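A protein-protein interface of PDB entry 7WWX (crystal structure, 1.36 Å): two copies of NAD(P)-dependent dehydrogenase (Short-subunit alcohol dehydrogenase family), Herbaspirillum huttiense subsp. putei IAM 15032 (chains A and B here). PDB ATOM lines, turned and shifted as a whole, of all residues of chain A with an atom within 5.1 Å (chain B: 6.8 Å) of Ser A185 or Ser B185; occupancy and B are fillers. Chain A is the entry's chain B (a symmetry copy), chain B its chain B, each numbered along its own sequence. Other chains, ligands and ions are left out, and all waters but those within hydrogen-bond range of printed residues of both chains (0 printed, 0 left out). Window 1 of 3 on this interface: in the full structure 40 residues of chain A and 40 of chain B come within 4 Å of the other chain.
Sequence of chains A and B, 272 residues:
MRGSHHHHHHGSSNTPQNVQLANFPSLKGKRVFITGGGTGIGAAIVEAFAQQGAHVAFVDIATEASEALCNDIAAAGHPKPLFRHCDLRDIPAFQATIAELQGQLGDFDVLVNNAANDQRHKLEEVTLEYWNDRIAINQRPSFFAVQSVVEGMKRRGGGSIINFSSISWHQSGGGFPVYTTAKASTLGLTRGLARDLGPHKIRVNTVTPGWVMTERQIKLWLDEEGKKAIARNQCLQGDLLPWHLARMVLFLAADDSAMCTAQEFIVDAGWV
Gln A139 touches Thr B181, and with the chains exchanged Thr A181 touches Gln B139.
Thr A181 touches Ser B185, and with the chains exchanged Ser A185 touches Thr B181.
Ala B184 touches its own counterpart, Ala A184.
Ala A184 touches Gly B188, and with the chains exchanged Gly A188 touches Ala B184.
Positions printed for both chains: 139, 180, 181, 182, 183, 184, 185, 186, 187, 188 and 189.
Of the 17 pairs that touch across the chains among the printed residues, 15 have their exchanged pair printed and touching as well.
Of chain B, only Thr B181 (3.5 Å) and Ser B185 (3.6 Å) come within 4 Å of Ser A185.
Of the printed residues of chain B, Leu A187 touches Trp B169.
Of the printed residues of chain A, Thr B180 touches Gly A188.
Thr B186 touches none of the printed residues of chain A.
Printed residues of chain A within 4 Å of Gly B188: Thr A180 (2.8 Å), Thr A181 (3.8 Å) and Ala A184 (3.3 Å).
The nearest residue of chain A that does not touch Ser B185 is Ala A184 (4.2 Å).
NE2 of Gln A139 touches CD1 of Ile B135 (3.8 Å).
Gln A139 touches Thr B181 (NE2 to CG2, 3.5 Å).
Gln B139 touches Thr A181 (NE2 to CG2, 3.5 Å).
O of Thr A181 touches CB of Ser B185 (3.5 Å).
Ala A184 touches Ala B184 (O to CB, 3.6 Å).
N of Gly B188 touches CB of Ala A184 (3.3 Å).
Ser A185 touches Thr B181 (CB to O, 3.5 Å).
Ser A185 touches Ser B185 (CB to CB, 3.6 Å).
CZ3 of Trp B169 touches CD2 of Leu A187, at 3.99 Å.
Thr B181 touches Leu A189 (OG1 to CA, 3.4 Å).
The side-chain hydroxyl of Ser B185 lies within hydrogen-bond range of the backbone carbonyl oxygen of Ala B182, at 2.7 Å.
The side-chain hydroxyl of Ser A185 lies close to the side-chain amide oxygen of Gln A139, 3.4 Å away.
The side-chain hydroxyl (OG) of Ser B165 is in hydrogen-bond range of the indole nitrogen (NE1) of Trp B169, 3.0 Å away.
O of Pro B177 is in hydrogen-bond range of OG1 of Thr B180 (3.0 Å).
The backbone carbonyl oxygen (O) of Pro B177 is in hydrogen-bond range of the side-chain hydroxyl (OG1) of Thr B181, at 2.7 Å.
OE1 of Gln B139 lies close to OG of Ser B185, at 3.4 Å.
OG1 of Thr B180 is in hydrogen-bond range of O of Gly A188 (2.8 Å).
The side-chain amide oxygen (OE1) of Gln B139 sits at hydrogen-bond distance from the side-chain amide nitrogen (NE2) of Gln A139.
The backbone carbonyl oxygen (O) of Gly B188 sits at hydrogen-bond distance from the side-chain hydroxyl (OG1) of Thr A180.
Hydrophobic or aromatic side chains of chain A within 4 Å of the printed part of chain B: Ala A184, Leu A187 and Leu A189.
Along chain A the printed residues that touch a printed residue of chain B span positions 139 to 189.
Printed residues of chain B that touch a printed residue of chain A: Ile B135, Gln B139, Trp B169, Thr B180, Thr B181, Ala B184, Ser B185, Gly B188 and Leu B189.
Hydrophobic or aromatic side chains of chain B within 4 Å of the printed part of chain A: Ile B135, Trp B169, Ala B184 and Leu B189.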
ATOM      1  N   GLN A 139      30.032  -9.008   6.916  1.00  0.00           N
ATOM      2  CA  GLN A 139      30.028  -7.555   6.637  1.00  0.00           C
ATOM      3  C   GLN A 139      30.225  -6.729   7.906  1.00  0.00           C
ATOM      4  O   GLN A 139      30.983  -5.751   7.908  1.00  0.00           O
ATOM      5  CB  GLN A 139      28.745  -7.207   5.866  1.00  0.00           C
ATOM      6  CG  GLN A 139      28.589  -5.773   5.460  1.00  0.00           C
ATOM      7  CD  GLN A 139      27.375  -5.544   4.594  1.00  0.00           C
ATOM      8  OE1 GLN A 139      26.987  -6.429   3.820  1.00  0.00           O
ATOM      9  NE2 GLN A 139      26.751  -4.411   4.795  1.00  0.00           N
ATOM     10  N   THR A 180      27.662 -12.744  -2.054  1.00  0.00           N
ATOM     11  CA  THR A 180      28.065 -11.784  -3.093  1.00  0.00           C
ATOM     12  C   THR A 180      27.684 -10.396  -2.609  1.00  0.00           C
ATOM     13  O   THR A 180      28.437  -9.429  -2.888  1.00  0.00           O
ATOM     14  CB  THR A 180      27.500 -12.137  -4.469  1.00  0.00           C
ATOM     15  OG1 THR A 180      26.070 -12.250  -4.442  1.00  0.00           O
ATOM     16  CG2 THR A 180      28.085 -13.436  -4.984  1.00  0.00           C
ATOM     17  N   THR A 181      26.517 -10.206  -2.003  1.00  0.00           N
ATOM     18  CA  THR A 181      26.102  -8.892  -1.482  1.00  0.00           C
ATOM     19  C   THR A 181      27.167  -8.359  -0.533  1.00  0.00           C
ATOM     20  O   THR A 181      27.648  -7.226  -0.633  1.00  0.00           O
ATOM     21  CB  THR A 181      24.736  -8.958  -0.783  1.00  0.00           C
ATOM     22  OG1 THR A 181      23.729  -9.397  -1.677  1.00  0.00           O
ATOM     23  CG2 THR A 181      24.373  -7.610  -0.233  1.00  0.00           C
ATOM     24  N   ALA A 182      27.535  -9.163   0.465  1.00  0.00           N
ATOM     25  CA  ALA A 182      28.482  -8.748   1.511  1.00  0.00           C
ATOM     26  C   ALA A 182      29.875  -8.512   0.906  1.00  0.00           C
ATOM     27  O   ALA A 182      30.576  -7.550   1.286  1.00  0.00           O
ATOM     28  CB  ALA A 182      28.538  -9.830   2.560  1.00  0.00           C
ATOM     29  N   LYS A 183      30.253  -9.299  -0.080  1.00  0.00           N
ATOM     30  CA  LYS A 183      31.592  -9.143  -0.682  1.00  0.00           C
ATOM     31  C   LYS A 183      31.686  -7.882  -1.527  1.00  0.00           C
ATOM     32  O   LYS A 183      32.729  -7.194  -1.482  1.00  0.00           O
ATOM     33  CB  LYS A 183      31.999 -10.387  -1.448  1.00  0.00           C
ATOM     34  CG  LYS A 183      32.245 -11.603  -0.594  1.00  0.00           C
ATOM     35  CD  LYS A 183      33.583 -11.561   0.097  1.00  0.00           C
ATOM     36  CE  LYS A 183      33.422 -11.266   1.553  1.00  0.00           C
ATOM     37  NZ  LYS A 183      34.748 -11.142   2.220  1.00  0.00           N
ATOM     38  N   ALA A 184      30.633  -7.506  -2.232  1.00  0.00           N
ATOM     39  CA  ALA A 184      30.604  -6.239  -2.984  1.00  0.00           C
ATOM     40  C   ALA A 184      30.602  -5.070  -2.001  1.00  0.00           C
ATOM     41  O   ALA A 184      31.201  -4.006  -2.270  1.00  0.00           O
ATOM     42  CB  ALA A 184      29.416  -6.193  -3.887  1.00  0.00           C
ATOM     43  N   SER A 185      29.937  -5.227  -0.858  1.00  0.00           N
ATOM     44  CA  SER A 185      29.802  -4.144   0.142  1.00  0.00           C
ATOM     45  C   SER A 185      31.186  -3.662   0.592  1.00  0.00           C
ATOM     46  O   SER A 185      31.335  -2.457   0.918  1.00  0.00           O
ATOM     47  CB  SER A 185      28.993  -4.593   1.341  1.00  0.00           C
ATOM     48  OG  SER A 185      29.765  -5.238   2.338  1.00  0.00           O
ATOM     49  N   THR A 186      32.189  -4.532   0.572  1.00  0.00           N
ATOM     50  CA  THR A 186      33.557  -4.177   0.993  1.00  0.00           C
ATOM     51  C   THR A 186      34.054  -2.972   0.215  1.00  0.00           C
ATOM     52  O   THR A 186      34.803  -2.114   0.775  1.00  0.00           O
ATOM     53  CB  THR A 186      34.501  -5.329   0.656  1.00  0.00           C
ATOM     54  OG1 THR A 186      33.951  -6.487   1.261  1.00  0.00           O
ATOM     55  CG2 THR A 186      35.918  -5.078   1.092  1.00  0.00           C
ATOM     56  N   LEU A 187      33.720  -2.871  -1.073  1.00  0.00           N
ATOM     57  CA  LEU A 187      34.240  -1.749  -1.876  1.00  0.00           C
ATOM     58  C   LEU A 187      33.676  -0.435  -1.351  1.00  0.00           C
ATOM     59  O   LEU A 187      34.386   0.587  -1.371  1.00  0.00           O
ATOM     60  CB  LEU A 187      33.904  -1.899  -3.357  1.00  0.00           C
ATOM     61  CG  LEU A 187      34.884  -2.788  -4.123  1.00  0.00           C
ATOM     62  CD1 LEU A 187      34.745  -4.251  -3.777  1.00  0.00           C
ATOM     63  CD2 LEU A 187      34.711  -2.573  -5.619  1.00  0.00           C
ATOM     64  N   GLY A 188      32.414  -0.427  -0.916  1.00  0.00           N
ATOM     65  CA  GLY A 188      31.821   0.801  -0.351  1.00  0.00           C
ATOM     66  C   GLY A 188      32.383   1.117   1.031  1.00  0.00           C
ATOM     67  O   GLY A 188      32.542   2.334   1.373  1.00  0.00           O
ATOM     68  N   LEU A 189      32.705   0.123   1.847  1.00  0.00           N
ATOM     69  CA  LEU A 189      33.355   0.370   3.133  1.00  0.00           C
ATOM     70  C   LEU A 189      34.727   0.999   2.892  1.00  0.00           C
ATOM     71  O   LEU A 189      35.056   2.028   3.462  1.00  0.00           O
ATOM     72  CB  LEU A 189      33.481  -0.932   3.930  1.00  0.00           C
ATOM     73  CG  LEU A 189      34.210  -0.790   5.253  1.00  0.00           C
ATOM     74  CD1 LEU A 189      33.380  -0.027   6.249  1.00  0.00           C
ATOM     75  CD2 LEU A 189      34.565  -2.140   5.811  1.00  0.00           C
ATOM     76  N   ILE B 135      21.516  -0.755   7.877  1.00  0.00           N
ATOM     77  CA  ILE B 135      21.484  -1.931   6.973  1.00  0.00           C
ATOM     78  C   ILE B 135      20.043  -2.415   6.827  1.00  0.00           C
ATOM     79  O   ILE B 135      19.607  -2.793   5.704  1.00  0.00           O
ATOM     80  CB  ILE B 135      22.476  -2.996   7.480  1.00  0.00           C
ATOM     81  CG1 ILE B 135      23.918  -2.465   7.377  1.00  0.00           C
ATOM     82  CG2 ILE B 135      22.278  -4.335   6.765  1.00  0.00           C
ATOM     83  CD1 ILE B 135      24.370  -1.811   6.086  1.00  0.00           C
ATOM     84  N   ASN B 138      18.677   0.215   4.256  1.00  0.00           N
ATOM     85  CA  ASN B 138      19.355   0.463   2.957  1.00  0.00           C
ATOM     86  C   ASN B 138      19.684  -0.831   2.216  1.00  0.00           C
ATOM     87  O   ASN B 138      19.888  -0.731   0.980  1.00  0.00           O
ATOM     88  CB  ASN B 138      20.618   1.284   3.147  1.00  0.00           C
ATOM     89  CG  ASN B 138      20.306   2.740   3.411  1.00  0.00           C
ATOM     90  OD1 ASN B 138      19.837   3.424   2.507  1.00  0.00           O
ATOM     91  ND2 ASN B 138      20.536   3.266   4.605  1.00  0.00           N
ATOM     92  N   GLN B 139      19.812  -1.983   2.871  1.00  0.00           N
ATOM     93  CA  GLN B 139      20.335  -3.210   2.231  1.00  0.00           C
ATOM     94  C   GLN B 139      19.357  -4.377   2.345  1.00  0.00           C
ATOM     95  O   GLN B 139      19.145  -5.116   1.376  1.00  0.00           O
ATOM     96  CB  GLN B 139      21.726  -3.511   2.810  1.00  0.00           C
ATOM     97  CG  GLN B 139      22.432  -4.706   2.244  1.00  0.00           C
ATOM     98  CD  GLN B 139      23.839  -4.850   2.767  1.00  0.00           C
ATOM     99  OE1 GLN B 139      24.503  -3.845   3.053  1.00  0.00           O
ATOM    100  NE2 GLN B 139      24.238  -6.081   2.965  1.00  0.00           N
ATOM    101  N   SER B 165      21.845   1.547  -6.761  1.00  0.00           N
ATOM    102  CA  SER B 165      23.099   1.902  -6.084  1.00  0.00           C
ATOM    103  C   SER B 165      23.184   3.426  -5.982  1.00  0.00           C
ATOM    104  O   SER B 165      22.157   4.095  -5.854  1.00  0.00           O
ATOM    105  CB  SER B 165      24.241   1.243  -6.763  1.00  0.00           C
ATOM    106  OG  SER B 165      25.466   1.427  -6.051  1.00  0.00           O
ATOM    107  N   TRP B 169      29.605   5.688  -3.538  1.00  0.00           N
ATOM    108  CA  TRP B 169      30.729   4.757  -3.303  1.00  0.00           C
ATOM    109  C   TRP B 169      31.762   4.887  -4.421  1.00  0.00           C
ATOM    110  O   TRP B 169      32.961   4.816  -4.189  1.00  0.00           O
ATOM    111  CB  TRP B 169      30.230   3.332  -3.092  1.00  0.00           C
ATOM    112  CG  TRP B 169      29.726   2.592  -4.269  1.00  0.00           C
ATOM    113  CD1 TRP B 169      28.442   2.512  -4.727  1.00  0.00           C
ATOM    114  CD2 TRP B 169      30.510   1.771  -5.132  1.00  0.00           C
ATOM    115  NE1 TRP B 169      28.395   1.700  -5.821  1.00  0.00           N
ATOM    116  CE2 TRP B 169      29.644   1.225  -6.101  1.00  0.00           C
ATOM    117  CE3 TRP B 169      31.871   1.422  -5.164  1.00  0.00           C
ATOM    118  CZ2 TRP B 169      30.082   0.380  -7.105  1.00  0.00           C
ATOM    119  CZ3 TRP B 169      32.294   0.561  -6.137  1.00  0.00           C
ATOM    120  CH2 TRP B 169      31.414   0.023  -7.061  1.00  0.00           C
ATOM    121  N   PRO B 177      29.898   6.215   5.952  1.00  0.00           N
ATOM    122  CA  PRO B 177      30.513   4.956   5.524  1.00  0.00           C
ATOM    123  C   PRO B 177      29.574   3.769   5.526  1.00  0.00           C
ATOM    124  O   PRO B 177      29.824   2.832   4.752  1.00  0.00           O
ATOM    125  CB  PRO B 177      31.683   4.740   6.481  1.00  0.00           C
ATOM    126  CG  PRO B 177      31.287   5.609   7.687  1.00  0.00           C
ATOM    127  CD  PRO B 177      30.625   6.819   7.070  1.00  0.00           C
ATOM    128  N   TYR B 179      26.407   3.921   4.684  1.00  0.00           N
ATOM    129  CA  TYR B 179      25.606   4.137   3.453  1.00  0.00           C
ATOM    130  C   TYR B 179      26.423   3.716   2.224  1.00  0.00           C
ATOM    131  O   TYR B 179      25.874   2.989   1.346  1.00  0.00           O
ATOM    132  CB  TYR B 179      25.221   5.601   3.341  1.00  0.00           C
ATOM    133  CG  TYR B 179      24.354   5.918   2.160  1.00  0.00           C
ATOM    134  CD1 TYR B 179      23.036   5.506   2.058  1.00  0.00           C
ATOM    135  CD2 TYR B 179      24.910   6.620   1.121  1.00  0.00           C
ATOM    136  CE1 TYR B 179      22.267   5.824   0.949  1.00  0.00           C
ATOM    137  CE2 TYR B 179      24.137   7.024   0.052  1.00  0.00           C
ATOM    138  CZ  TYR B 179      22.821   6.597  -0.054  1.00  0.00           C
ATOM    139  OH  TYR B 179      22.126   6.980  -1.205  1.00  0.00           O
ATOM    140  N   THR B 180      27.678   4.147   2.112  1.00  0.00           N
ATOM    141  CA  THR B 180      28.506   3.723   0.972  1.00  0.00           C
ATOM    142  C   THR B 180      28.594   2.208   1.006  1.00  0.00           C
ATOM    143  O   THR B 180      28.613   1.577  -0.081  1.00  0.00           O
ATOM    144  CB  THR B 180      29.866   4.422   0.942  1.00  0.00           C
ATOM    145  OG1 THR B 180      30.589   4.228   2.165  1.00  0.00           O
ATOM    146  CG2 THR B 180      29.711   5.909   0.695  1.00  0.00           C
ATOM    147  N   THR B 181      28.763   1.583   2.167  1.00  0.00           N
ATOM    148  CA  THR B 181      28.824   0.115   2.272  1.00  0.00           C
ATOM    149  C   THR B 181      27.582  -0.495   1.637  1.00  0.00           C
ATOM    150  O   THR B 181      27.634  -1.396   0.793  1.00  0.00           O
ATOM    151  CB  THR B 181      28.972  -0.350   3.729  1.00  0.00           C
ATOM    152  OG1 THR B 181      30.158   0.167   4.308  1.00  0.00           O
ATOM    153  CG2 THR B 181      28.989  -1.849   3.792  1.00  0.00           C
ATOM    154  N   ALA B 182      26.405  -0.043   2.071  1.00  0.00           N
ATOM    155  CA  ALA B 182      25.123  -0.605   1.617  1.00  0.00           C
ATOM    156  C   ALA B 182      24.918  -0.324   0.121  1.00  0.00           C
ATOM    157  O   ALA B 182      24.424  -1.195  -0.626  1.00  0.00           O
ATOM    158  CB  ALA B 182      24.016   0.020   2.429  1.00  0.00           C
ATOM    159  N   LYS B 183      25.363   0.823  -0.352  1.00  0.00           N
ATOM    160  CA  LYS B 183      25.169   1.165  -1.774  1.00  0.00           C
ATOM    161  C   LYS B 183      26.064   0.335  -2.681  1.00  0.00           C
ATOM    162  O   LYS B 183      25.605  -0.099  -3.760  1.00  0.00           O
ATOM    163  CB  LYS B 183      25.326   2.655  -2.009  1.00  0.00           C
ATOM    164  CG  LYS B 183      24.250   3.509  -1.392  1.00  0.00           C
ATOM    165  CD  LYS B 183      22.973   3.494  -2.192  1.00  0.00           C
ATOM    166  CE  LYS B 183      21.927   2.673  -1.511  1.00  0.00           C
ATOM    167  NZ  LYS B 183      20.693   2.589  -2.341  1.00  0.00           N
ATOM    168  N   ALA B 184      27.282   0.031  -2.270  1.00  0.00           N
ATOM    169  CA  ALA B 184      28.169  -0.863  -3.036  1.00  0.00           C
ATOM    170  C   ALA B 184      27.601  -2.280  -3.010  1.00  0.00           C
ATOM    171  O   ALA B 184      27.714  -3.034  -4.000  1.00  0.00           O
ATOM    172  CB  ALA B 184      29.557  -0.822  -2.486  1.00  0.00           C
ATOM    173  N   SER B 185      26.991  -2.679  -1.895  1.00  0.00           N
ATOM    174  CA  SER B 185      26.462  -4.050  -1.722  1.00  0.00           C
ATOM    175  C   SER B 185      25.448  -4.372  -2.824  1.00  0.00           C
ATOM    176  O   SER B 185      25.343  -5.557  -3.230  1.00  0.00           O
ATOM    177  CB  SER B 185      25.825  -4.231  -0.360  1.00  0.00           C
ATOM    178  OG  SER B 185      24.464  -3.843  -0.313  1.00  0.00           O
ATOM    179  N   THR B 186      24.750  -3.369  -3.344  1.00  0.00           N
ATOM    180  CA  THR B 186      23.741  -3.568  -4.402  1.00  0.00           C
ATOM    181  C   THR B 186      24.354  -4.289  -5.589  1.00  0.00           C
ATOM    182  O   THR B 186      23.666  -5.121  -6.256  1.00  0.00           O
ATOM    183  CB  THR B 186      23.278  -2.205  -4.916  1.00  0.00           C
ATOM    184  OG1 THR B 186      22.845  -1.476  -3.780  1.00  0.00           O
ATOM    185  CG2 THR B 186      22.210  -2.304  -5.969  1.00  0.00           C
ATOM    186  N   LEU B 187      25.609  -3.989  -5.930  1.00  0.00           N
ATOM    187  CA  LEU B 187      26.213  -4.621  -7.117  1.00  0.00           C
ATOM    188  C   LEU B 187      26.351  -6.121  -6.888  1.00  0.00           C
ATOM    189  O   LEU B 187      26.192  -6.903  -7.843  1.00  0.00           O
ATOM    190  CB  LEU B 187      27.576  -4.023  -7.455  1.00  0.00           C
ATOM    191  CG  LEU B 187      27.498  -2.742  -8.284  1.00  0.00           C
ATOM    192  CD1 LEU B 187      26.994  -1.558  -7.493  1.00  0.00           C
ATOM    193  CD2 LEU B 187      28.859  -2.440  -8.892  1.00  0.00           C
ATOM    194  N   GLY B 188      26.674  -6.538  -5.662  1.00  0.00           N
ATOM    195  CA  GLY B 188      26.778  -7.979  -5.360  1.00  0.00           C
ATOM    196  C   GLY B 188      25.408  -8.647  -5.311  1.00  0.00           C
ATOM    197  O   GLY B 188      25.287  -9.847  -5.722  1.00  0.00           O
ATOM    198  N   LEU B 189      24.366  -7.966  -4.854  1.00  0.00           N
ATOM    199  CA  LEU B 189      23.014  -8.519  -4.897  1.00  0.00           C
ATOM    200  C   LEU B 189      22.600  -8.730  -6.352  1.00  0.00           C
ATOM    201  O   LEU B 189      22.164  -9.806  -6.733  1.00  0.00           O
ATOM    202  CB  LEU B 189      22.031  -7.591  -4.177  1.00  0.00           C
ATOM    203  CG  LEU B 189      20.584  -8.045  -4.230  1.00  0.00           C
ATOM    204  CD1 LEU B 189      20.369  -9.263  -3.374  1.00  0.00           C
ATOM    205  CD2 LEU B 189      19.664  -6.941  -3.788  1.00  0.00           C
ATOM    206  N   THR B 190      22.787  -7.728  -7.157  1.00  0.00           N
ATOM    207  CA  THR B 190      22.413  -7.758  -8.577  1.00  0.00           C
ATOM    208  C   THR B 190      23.129  -8.930  -9.237  1.00  0.00           C
ATOM    209  O   THR B 190      22.504  -9.716  -9.989  1.00  0.00           O
ATOM    210  CB  THR B 190      22.766  -6.442  -9.291  1.00  0.00           C
ATOM    211  OG1 THR B 190      21.863  -5.441  -8.824  1.00  0.00           O
ATOM    212  CG2 THR B 190      22.672  -6.584 -10.788  1.00  0.00           C
